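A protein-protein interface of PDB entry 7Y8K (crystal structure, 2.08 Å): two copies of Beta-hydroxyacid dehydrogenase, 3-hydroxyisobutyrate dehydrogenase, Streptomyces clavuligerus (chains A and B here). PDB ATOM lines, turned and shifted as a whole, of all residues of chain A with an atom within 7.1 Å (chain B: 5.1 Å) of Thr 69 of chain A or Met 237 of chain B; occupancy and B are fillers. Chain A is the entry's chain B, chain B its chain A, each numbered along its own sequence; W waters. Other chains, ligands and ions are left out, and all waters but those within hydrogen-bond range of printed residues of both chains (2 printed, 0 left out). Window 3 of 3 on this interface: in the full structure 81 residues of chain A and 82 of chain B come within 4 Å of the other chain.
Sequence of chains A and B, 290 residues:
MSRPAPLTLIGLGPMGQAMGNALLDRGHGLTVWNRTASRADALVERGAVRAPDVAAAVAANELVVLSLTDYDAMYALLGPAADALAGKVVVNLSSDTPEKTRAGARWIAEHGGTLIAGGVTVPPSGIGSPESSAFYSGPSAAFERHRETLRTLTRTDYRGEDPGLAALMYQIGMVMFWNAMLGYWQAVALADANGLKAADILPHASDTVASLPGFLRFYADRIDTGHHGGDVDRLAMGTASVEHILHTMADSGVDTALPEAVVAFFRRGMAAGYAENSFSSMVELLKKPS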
ATOM      1  N   PRO A  14      -0.343 -26.274  30.680  1.00  0.00           N
ATOM      2  CA  PRO A  14      -0.684 -27.102  31.843  1.00  0.00           C
ATOM      3  C   PRO A  14      -0.620 -28.623  31.589  1.00  0.00           C
ATOM      4  O   PRO A  14       0.008 -29.307  32.359  1.00  0.00           O
ATOM      5  CB  PRO A  14      -2.115 -26.641  32.162  1.00  0.00           C
ATOM      6  CG  PRO A  14      -2.146 -25.200  31.722  1.00  0.00           C
ATOM      7  CD  PRO A  14      -1.261 -25.152  30.495  1.00  0.00           C
ATOM      8  N   SER A  67       1.533 -31.453  22.825  1.00  0.00           N
ATOM      9  CA  SER A  67       0.361 -30.982  23.602  1.00  0.00           C
ATOM     10  C   SER A  67       0.153 -29.507  23.250  1.00  0.00           C
ATOM     11  O   SER A  67       0.616 -28.647  23.990  1.00  0.00           O
ATOM     12  CB  SER A  67       0.457 -31.226  25.086  1.00  0.00           C
ATOM     13  OG  SER A  67      -0.728 -30.837  25.745  1.00  0.00           O
ATOM     14  N   LEU A  68      -0.537 -29.254  22.146  1.00  0.00           N
ATOM     15  CA  LEU A  68      -0.812 -27.876  21.673  1.00  0.00           C
ATOM     16  C   LEU A  68      -2.316 -27.632  21.538  1.00  0.00           C
ATOM     17  O   LEU A  68      -3.098 -28.560  21.761  1.00  0.00           O
ATOM     18  CB  LEU A  68      -0.090 -27.666  20.338  1.00  0.00           C
ATOM     19  CG  LEU A  68       1.406 -27.961  20.321  1.00  0.00           C
ATOM     20  CD1 LEU A  68       1.890 -28.190  18.903  1.00  0.00           C
ATOM     21  CD2 LEU A  68       2.180 -26.834  20.976  1.00  0.00           C
ATOM     22  N   THR A  69      -2.698 -26.411  21.167  1.00  0.00           N
ATOM     23  CA  THR A  69      -4.124 -26.024  21.084  1.00  0.00           C
ATOM     24  C   THR A  69      -4.852 -26.823  20.012  1.00  0.00           C
ATOM     25  O   THR A  69      -5.953 -27.321  20.291  1.00  0.00           O
ATOM     26  CB  THR A  69      -4.234 -24.534  20.728  1.00  0.00           C
ATOM     27  OG1 THR A  69      -3.543 -23.760  21.709  1.00  0.00           O
ATOM     28  CG2 THR A  69      -5.662 -24.047  20.582  1.00  0.00           C
ATOM     29  N   ASP A  70      -4.242 -26.927  18.837  1.00  0.00           N
ATOM     30  CA  ASP A  70      -4.898 -27.600  17.700  1.00  0.00           C
ATOM     31  C   ASP A  70      -3.823 -28.185  16.783  1.00  0.00           C
ATOM     32  O   ASP A  70      -2.659 -28.248  17.191  1.00  0.00           O
ATOM     33  CB  ASP A  70      -5.816 -26.606  16.992  1.00  0.00           C
ATOM     34  CG  ASP A  70      -5.203 -25.241  16.713  1.00  0.00           C
ATOM     35  OD1 ASP A  70      -4.012 -25.176  16.395  1.00  0.00           O
ATOM     36  OD2 ASP A  70      -5.930 -24.252  16.811  1.00  0.00           O
ATOM     37  N   TYR A  71      -4.213 -28.556  15.570  1.00  0.00           N
ATOM     38  CA  TYR A  71      -3.261 -29.136  14.596  1.00  0.00           C
ATOM     39  C   TYR A  71      -2.619 -27.991  13.825  1.00  0.00           C
ATOM     40  O   TYR A  71      -1.472 -28.136  13.436  1.00  0.00           O
ATOM     41  CB  TYR A  71      -3.971 -30.185  13.740  1.00  0.00           C
ATOM     42  CG  TYR A  71      -3.868 -31.585  14.279  1.00  0.00           C
ATOM     43  CD1 TYR A  71      -4.366 -31.908  15.530  1.00  0.00           C
ATOM     44  CD2 TYR A  71      -3.247 -32.580  13.549  1.00  0.00           C
ATOM     45  CE1 TYR A  71      -4.265 -33.192  16.035  1.00  0.00           C
ATOM     46  CE2 TYR A  71      -3.133 -33.868  14.040  1.00  0.00           C
ATOM     47  CZ  TYR A  71      -3.646 -34.174  15.285  1.00  0.00           C
ATOM     48  OH  TYR A  71      -3.533 -35.438  15.768  1.00  0.00           O
ATOM     49  N   ASP A  72      -3.353 -26.898  13.613  1.00  0.00           N
ATOM     50  CA  ASP A  72      -2.762 -25.686  12.987  1.00  0.00           C
ATOM     51  C   ASP A  72      -1.477 -25.332  13.728  1.00  0.00           C
ATOM     52  O   ASP A  72      -0.485 -25.038  13.070  1.00  0.00           O
ATOM     53  CB  ASP A  72      -3.748 -24.527  13.027  1.00  0.00           C
ATOM     54  CG  ASP A  72      -4.710 -24.509  11.853  1.00  0.00           C
ATOM     55  OD1 ASP A  72      -4.434 -25.196  10.860  1.00  0.00           O
ATOM     56  OD2 ASP A  72      -5.728 -23.815  11.950  1.00  0.00           O
ATOM     57  N   ALA A  73      -1.511 -25.411  15.049  1.00  0.00           N
ATOM     58  CA  ALA A  73      -0.318 -25.160  15.885  1.00  0.00           C
ATOM     59  C   ALA A  73       0.831 -26.107  15.524  1.00  0.00           C
ATOM     60  O   ALA A  73       1.960 -25.620  15.431  1.00  0.00           O
ATOM     61  CB  ALA A  73      -0.692 -25.262  17.336  1.00  0.00           C
ATOM     62  N   MET A  74       0.552 -27.385  15.299  1.00  0.00           N
ATOM     63  CA  MET A  74       1.616 -28.333  14.890  1.00  0.00           C
ATOM     64  C   MET A  74       2.314 -27.813  13.635  1.00  0.00           C
ATOM     65  O   MET A  74       3.536 -27.696  13.654  1.00  0.00           O
ATOM     66  CB  MET A  74       1.058 -29.730  14.603  1.00  0.00           C
ATOM     67  CG  MET A  74       2.107 -30.727  14.200  1.00  0.00           C
ATOM     68  SD  MET A  74       1.393 -32.347  13.904  1.00  0.00           S
ATOM     69  CE  MET A  74       0.591 -32.057  12.332  1.00  0.00           C
ATOM     70  N   SER A  94      -3.316 -33.308  20.885  1.00  0.00           N
ATOM     71  CA  SER A  94      -4.017 -32.017  20.731  1.00  0.00           C
ATOM     72  C   SER A  94      -5.472 -32.230  20.279  1.00  0.00           C
ATOM     73  O   SER A  94      -5.705 -33.013  19.362  1.00  0.00           O
ATOM     74  CB  SER A  94      -3.241 -31.118  19.786  1.00  0.00           C
ATOM     75  OG  SER A  94      -1.907 -30.920  20.218  1.00  0.00           O
ATOM     76  N   SER A  95      -6.403 -31.536  20.932  1.00  0.00           N
ATOM     77  CA  SER A  95      -7.823 -31.607  20.515  1.00  0.00           C
ATOM     78  C   SER A  95      -7.999 -30.982  19.139  1.00  0.00           C
ATOM     79  O   SER A  95      -7.375 -29.950  18.890  1.00  0.00           O
ATOM     80  CB  SER A  95      -8.765 -30.950  21.476  1.00  0.00           C
ATOM     81  OG  SER A  95     -10.053 -30.773  20.910  1.00  0.00           O
ATOM     82  N   ASP A  96      -8.823 -31.617  18.326  1.00  0.00           N
ATOM     83  CA  ASP A  96      -9.175 -31.086  16.992  1.00  0.00           C
ATOM     84  C   ASP A  96     -10.247 -31.970  16.350  1.00  0.00           C
ATOM     85  O   ASP A  96     -10.594 -32.997  16.923  1.00  0.00           O
ATOM     86  CB  ASP A  96      -7.982 -30.963  16.044  1.00  0.00           C
ATOM     87  CG  ASP A  96      -8.024 -29.694  15.204  1.00  0.00           C
ATOM     88  OD1 ASP A  96      -9.096 -29.369  14.688  1.00  0.00           O
ATOM     89  OD2 ASP A  96      -6.989 -29.049  15.068  1.00  0.00           O
ATOM     90  N   TRP A 178     -19.382 -30.463  28.449  1.00  0.00           N
ATOM     91  CA  TRP A 178     -19.741 -29.026  28.326  1.00  0.00           C
ATOM     92  C   TRP A 178     -21.238 -28.804  28.531  1.00  0.00           C
ATOM     93  O   TRP A 178     -21.558 -27.909  29.262  1.00  0.00           O
ATOM     94  CB  TRP A 178     -19.238 -28.475  27.000  1.00  0.00           C
ATOM     95  CG  TRP A 178     -17.757 -28.485  26.804  1.00  0.00           C
ATOM     96  CD1 TRP A 178     -17.089 -29.066  25.772  1.00  0.00           C
ATOM     97  CD2 TRP A 178     -16.755 -27.866  27.627  1.00  0.00           C
ATOM     98  NE1 TRP A 178     -15.747 -28.862  25.896  1.00  0.00           N
ATOM     99  CE2 TRP A 178     -15.509 -28.127  27.021  1.00  0.00           C
ATOM    100  CE3 TRP A 178     -16.779 -27.123  28.810  1.00  0.00           C
ATOM    101  CZ2 TRP A 178     -14.308 -27.681  27.563  1.00  0.00           C
ATOM    102  CZ3 TRP A 178     -15.590 -26.682  29.344  1.00  0.00           C
ATOM    103  CH2 TRP A 178     -14.372 -26.959  28.730  1.00  0.00           C
ATOM    104  N   ARG B 234      -8.807 -22.976  31.248  1.00  0.00           N
ATOM    105  CA  ARG B 234      -8.868 -21.641  30.684  1.00  0.00           C
ATOM    106  C   ARG B 234      -9.999 -21.577  29.667  1.00  0.00           C
ATOM    107  O   ARG B 234     -10.030 -22.380  28.734  1.00  0.00           O
ATOM    108  CB  ARG B 234      -7.531 -21.270  30.037  1.00  0.00           C
ATOM    109  CG  ARG B 234      -6.371 -21.279  31.044  1.00  0.00           C
ATOM    110  CD  ARG B 234      -5.844 -19.865  31.237  1.00  0.00           C
ATOM    111  NE  ARG B 234      -5.337 -19.607  32.586  1.00  0.00           N
ATOM    112  CZ  ARG B 234      -4.116 -19.930  32.986  1.00  0.00           C
ATOM    113  NH1 ARG B 234      -3.291 -20.615  32.207  1.00  0.00           N
ATOM    114  NH2 ARG B 234      -3.704 -19.543  34.191  1.00  0.00           N
ATOM    115  N   LEU B 235     -10.914 -20.623  29.851  1.00  0.00           N
ATOM    116  CA  LEU B 235     -11.952 -20.319  28.868  1.00  0.00           C
ATOM    117  C   LEU B 235     -11.449 -20.372  27.433  1.00  0.00           C
ATOM    118  O   LEU B 235     -12.123 -20.920  26.552  1.00  0.00           O
ATOM    119  CB  LEU B 235     -12.536 -18.936  29.125  1.00  0.00           C
ATOM    120  CG  LEU B 235     -13.755 -18.599  28.283  1.00  0.00           C
ATOM    121  CD1 LEU B 235     -14.782 -19.741  28.304  1.00  0.00           C
ATOM    122  CD2 LEU B 235     -14.378 -17.322  28.756  1.00  0.00           C
ATOM    123  N   ALA B 236     -10.268 -19.795  27.186  1.00  0.00           N
ATOM    124  CA  ALA B 236      -9.674 -19.854  25.851  1.00  0.00           C
ATOM    125  C   ALA B 236      -9.593 -21.287  25.328  1.00  0.00           C
ATOM    126  O   ALA B 236      -9.842 -21.544  24.144  1.00  0.00           O
ATOM    127  CB  ALA B 236      -8.280 -19.222  25.882  1.00  0.00           C
ATOM    128  N   MET B 237      -9.235 -22.232  26.198  1.00  0.00           N
ATOM    129  CA  MET B 237      -9.198 -23.636  25.805  1.00  0.00           C
ATOM    130  C   MET B 237     -10.603 -24.218  25.714  1.00  0.00           C
ATOM    131  O   MET B 237     -10.876 -25.071  24.862  1.00  0.00           O
ATOM    132  CB  MET B 237      -8.368 -24.448  26.804  1.00  0.00           C
ATOM    133  CG  MET B 237      -6.867 -24.321  26.651  1.00  0.00           C
ATOM    134  SD  MET B 237      -6.218 -25.299  25.274  1.00  0.00           S
ATOM    135  CE  MET B 237      -5.675 -23.997  24.165  1.00  0.00           C
ATOM    136  N   GLY B 238     -11.494 -23.810  26.615  1.00  0.00           N
ATOM    137  CA  GLY B 238     -12.865 -24.274  26.517  1.00  0.00           C
ATOM    138  C   GLY B 238     -13.506 -23.850  25.212  1.00  0.00           C
ATOM    139  O   GLY B 238     -14.166 -24.651  24.540  1.00  0.00           O
ATOM    140  N   THR B 239     -13.299 -22.585  24.822  1.00  0.00           N
ATOM    141  CA  THR B 239     -13.834 -22.087  23.556  1.00  0.00           C
ATOM    142  C   THR B 239     -13.284 -22.871  22.373  1.00  0.00           C
ATOM    143  O   THR B 239     -14.036 -23.246  21.461  1.00  0.00           O
ATOM    144  CB  THR B 239     -13.522 -20.601  23.383  1.00  0.00           C
ATOM    145  OG1 THR B 239     -13.935 -19.890  24.554  1.00  0.00           O
ATOM    146  CG2 THR B 239     -14.268 -20.036  22.144  1.00  0.00           C
ATOM    147  N   ALA B 240     -11.974 -23.114  22.364  1.00  0.00           N
ATOM    148  CA  ALA B 240     -11.389 -23.937  21.319  1.00  0.00           C
ATOM    149  C   ALA B 240     -12.082 -25.290  21.258  1.00  0.00           C
ATOM    150  O   ALA B 240     -12.371 -25.812  20.173  1.00  0.00           O
ATOM    151  CB  ALA B 240      -9.888 -24.096  21.567  1.00  0.00           C
ATOM    152  N   SER B 241     -12.405 -25.844  22.424  1.00  0.00           N
ATOM    153  CA  SER B 241     -12.960 -27.187  22.481  1.00  0.00           C
ATOM    154  C   SER B 241     -14.392 -27.221  21.957  1.00  0.00           C
ATOM    155  O   SER B 241     -14.773 -28.150  21.231  1.00  0.00           O
ATOM    156  CB  SER B 241     -12.891 -27.701  23.914  1.00  0.00           C
ATOM    157  OG  SER B 241     -13.481 -28.979  24.010  1.00  0.00           O
ATOM    158  N   HIS B 244     -14.237 -27.025  18.198  1.00  0.00           N
ATOM    159  CA  HIS B 244     -13.907 -28.312  17.580  1.00  0.00           C
ATOM    160  C   HIS B 244     -15.092 -29.270  17.594  1.00  0.00           C
ATOM    161  O   HIS B 244     -15.210 -30.114  16.698  1.00  0.00           O
ATOM    162  CB  HIS B 244     -12.716 -28.973  18.295  1.00  0.00           C
ATOM    163  CG  HIS B 244     -11.463 -28.143  18.292  1.00  0.00           C
ATOM    164  ND1 HIS B 244     -10.416 -28.369  19.160  1.00  0.00           N
ATOM    165  CD2 HIS B 244     -11.096 -27.082  17.535  1.00  0.00           C
ATOM    166  CE1 HIS B 244      -9.455 -27.494  18.932  1.00  0.00           C
ATOM    167  NE2 HIS B 244      -9.842 -26.703  17.948  1.00  0.00           N
HETATM  168  O   HOH W   1     -12.735 -30.487  22.018  1.00  0.00           O
HETATM  169  O   HOH W   2      -8.450 -24.500  17.099  1.00  0.00           O
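OG of Ser 241 of chain B lies within hydrogen-bond range of NE1 of Trp 178 of chain A (3.0 Å).
ND1 of His 244 of chain B sits at hydrogen-bond distance from OG of Ser 95 of chain A (3.0 Å).
The backbone carbonyl oxygen (O) of Ala 240 of chain B lies close to a ring nitrogen (ND1) of His 244 of chain B (3.4 Å).
The backbone NH (N) of Tyr 71 of chain A lies within hydrogen-bond range of the side-chain carboxylate (OD2) of Asp 96 of chain A (2.9 Å).
Among the printed residues, pairs that only touch across the chains: Thr 69 of chain A with Met 237 of chain B (3.3 Å), Thr 69 of chain A with His 244 of chain B (3.8 Å), Asp 96 of chain A with His 244 of chain B (3.7 Å) and Trp 178 of chain A with Gly 238 of chain B (3.8 Å).
Thr 69 of chain A touches just these residues of chain B: Met 237 (3.3 Å) and His 244 (3.8 Å).
Asp 70 of chain A touches none of the printed residues of chain B.
Printed residues of chain B within 4 Å of Ser 95 of chain A: His 244 (3.0 Å).
Of the printed residues of chain B, Asp 96 of chain A touches His 244.
Printed residues of chain B within 4 Å of Trp 178 of chain A: Gly 238 (3.8 Å) and Ser 241 (3.0 Å).
Leu 235 of chain B touches none of the printed residues of chain A.
Of the printed residues of chain A, Gly 238 of chain B touches Trp 178 (3.8 Å).
Of the printed residues of chain A, His 244 of chain B touches Thr 69, Ser 95 and Asp 96.
The nearest residue of chain B that does not touch Thr 69 of chain A is Ala 240 of chain B (4.3 Å).
Hydrophobic or aromatic side chains of chain B within 4 Å of the printed part of chain A: Met 237 and His 244.
Printed residues of chain A that touch a printed residue of chain B: Thr 69, Ser 95, Asp 96 and Trp 178.
Hydrophobic or aromatic side chains of chain A within 4 Å of the printed part of chain B: Trp 178.
Among the printed residues, 6 pairs touch across the chains.
Among the printed residues, no Asp or Glu carboxylate lies within 4 Å of a Lys or Arg side-chain nitrogen of the other chain.
No position is printed for both chains.
Of the 6 pairs that touch across the chains among the printed residues, none has its exchanged pair printed and touching as well.
Water W2 bridges OD2 of Asp 70 of chain A (2.5 Å) and NE2 of His 244 of chain B (2.7 Å).
Water W1 lies within hydrogen-bond range of the side-chain hydroxyl (OG) of Ser 241 of chain B and the side-chain hydroxyl (OG) of Ser 95 of chain A.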
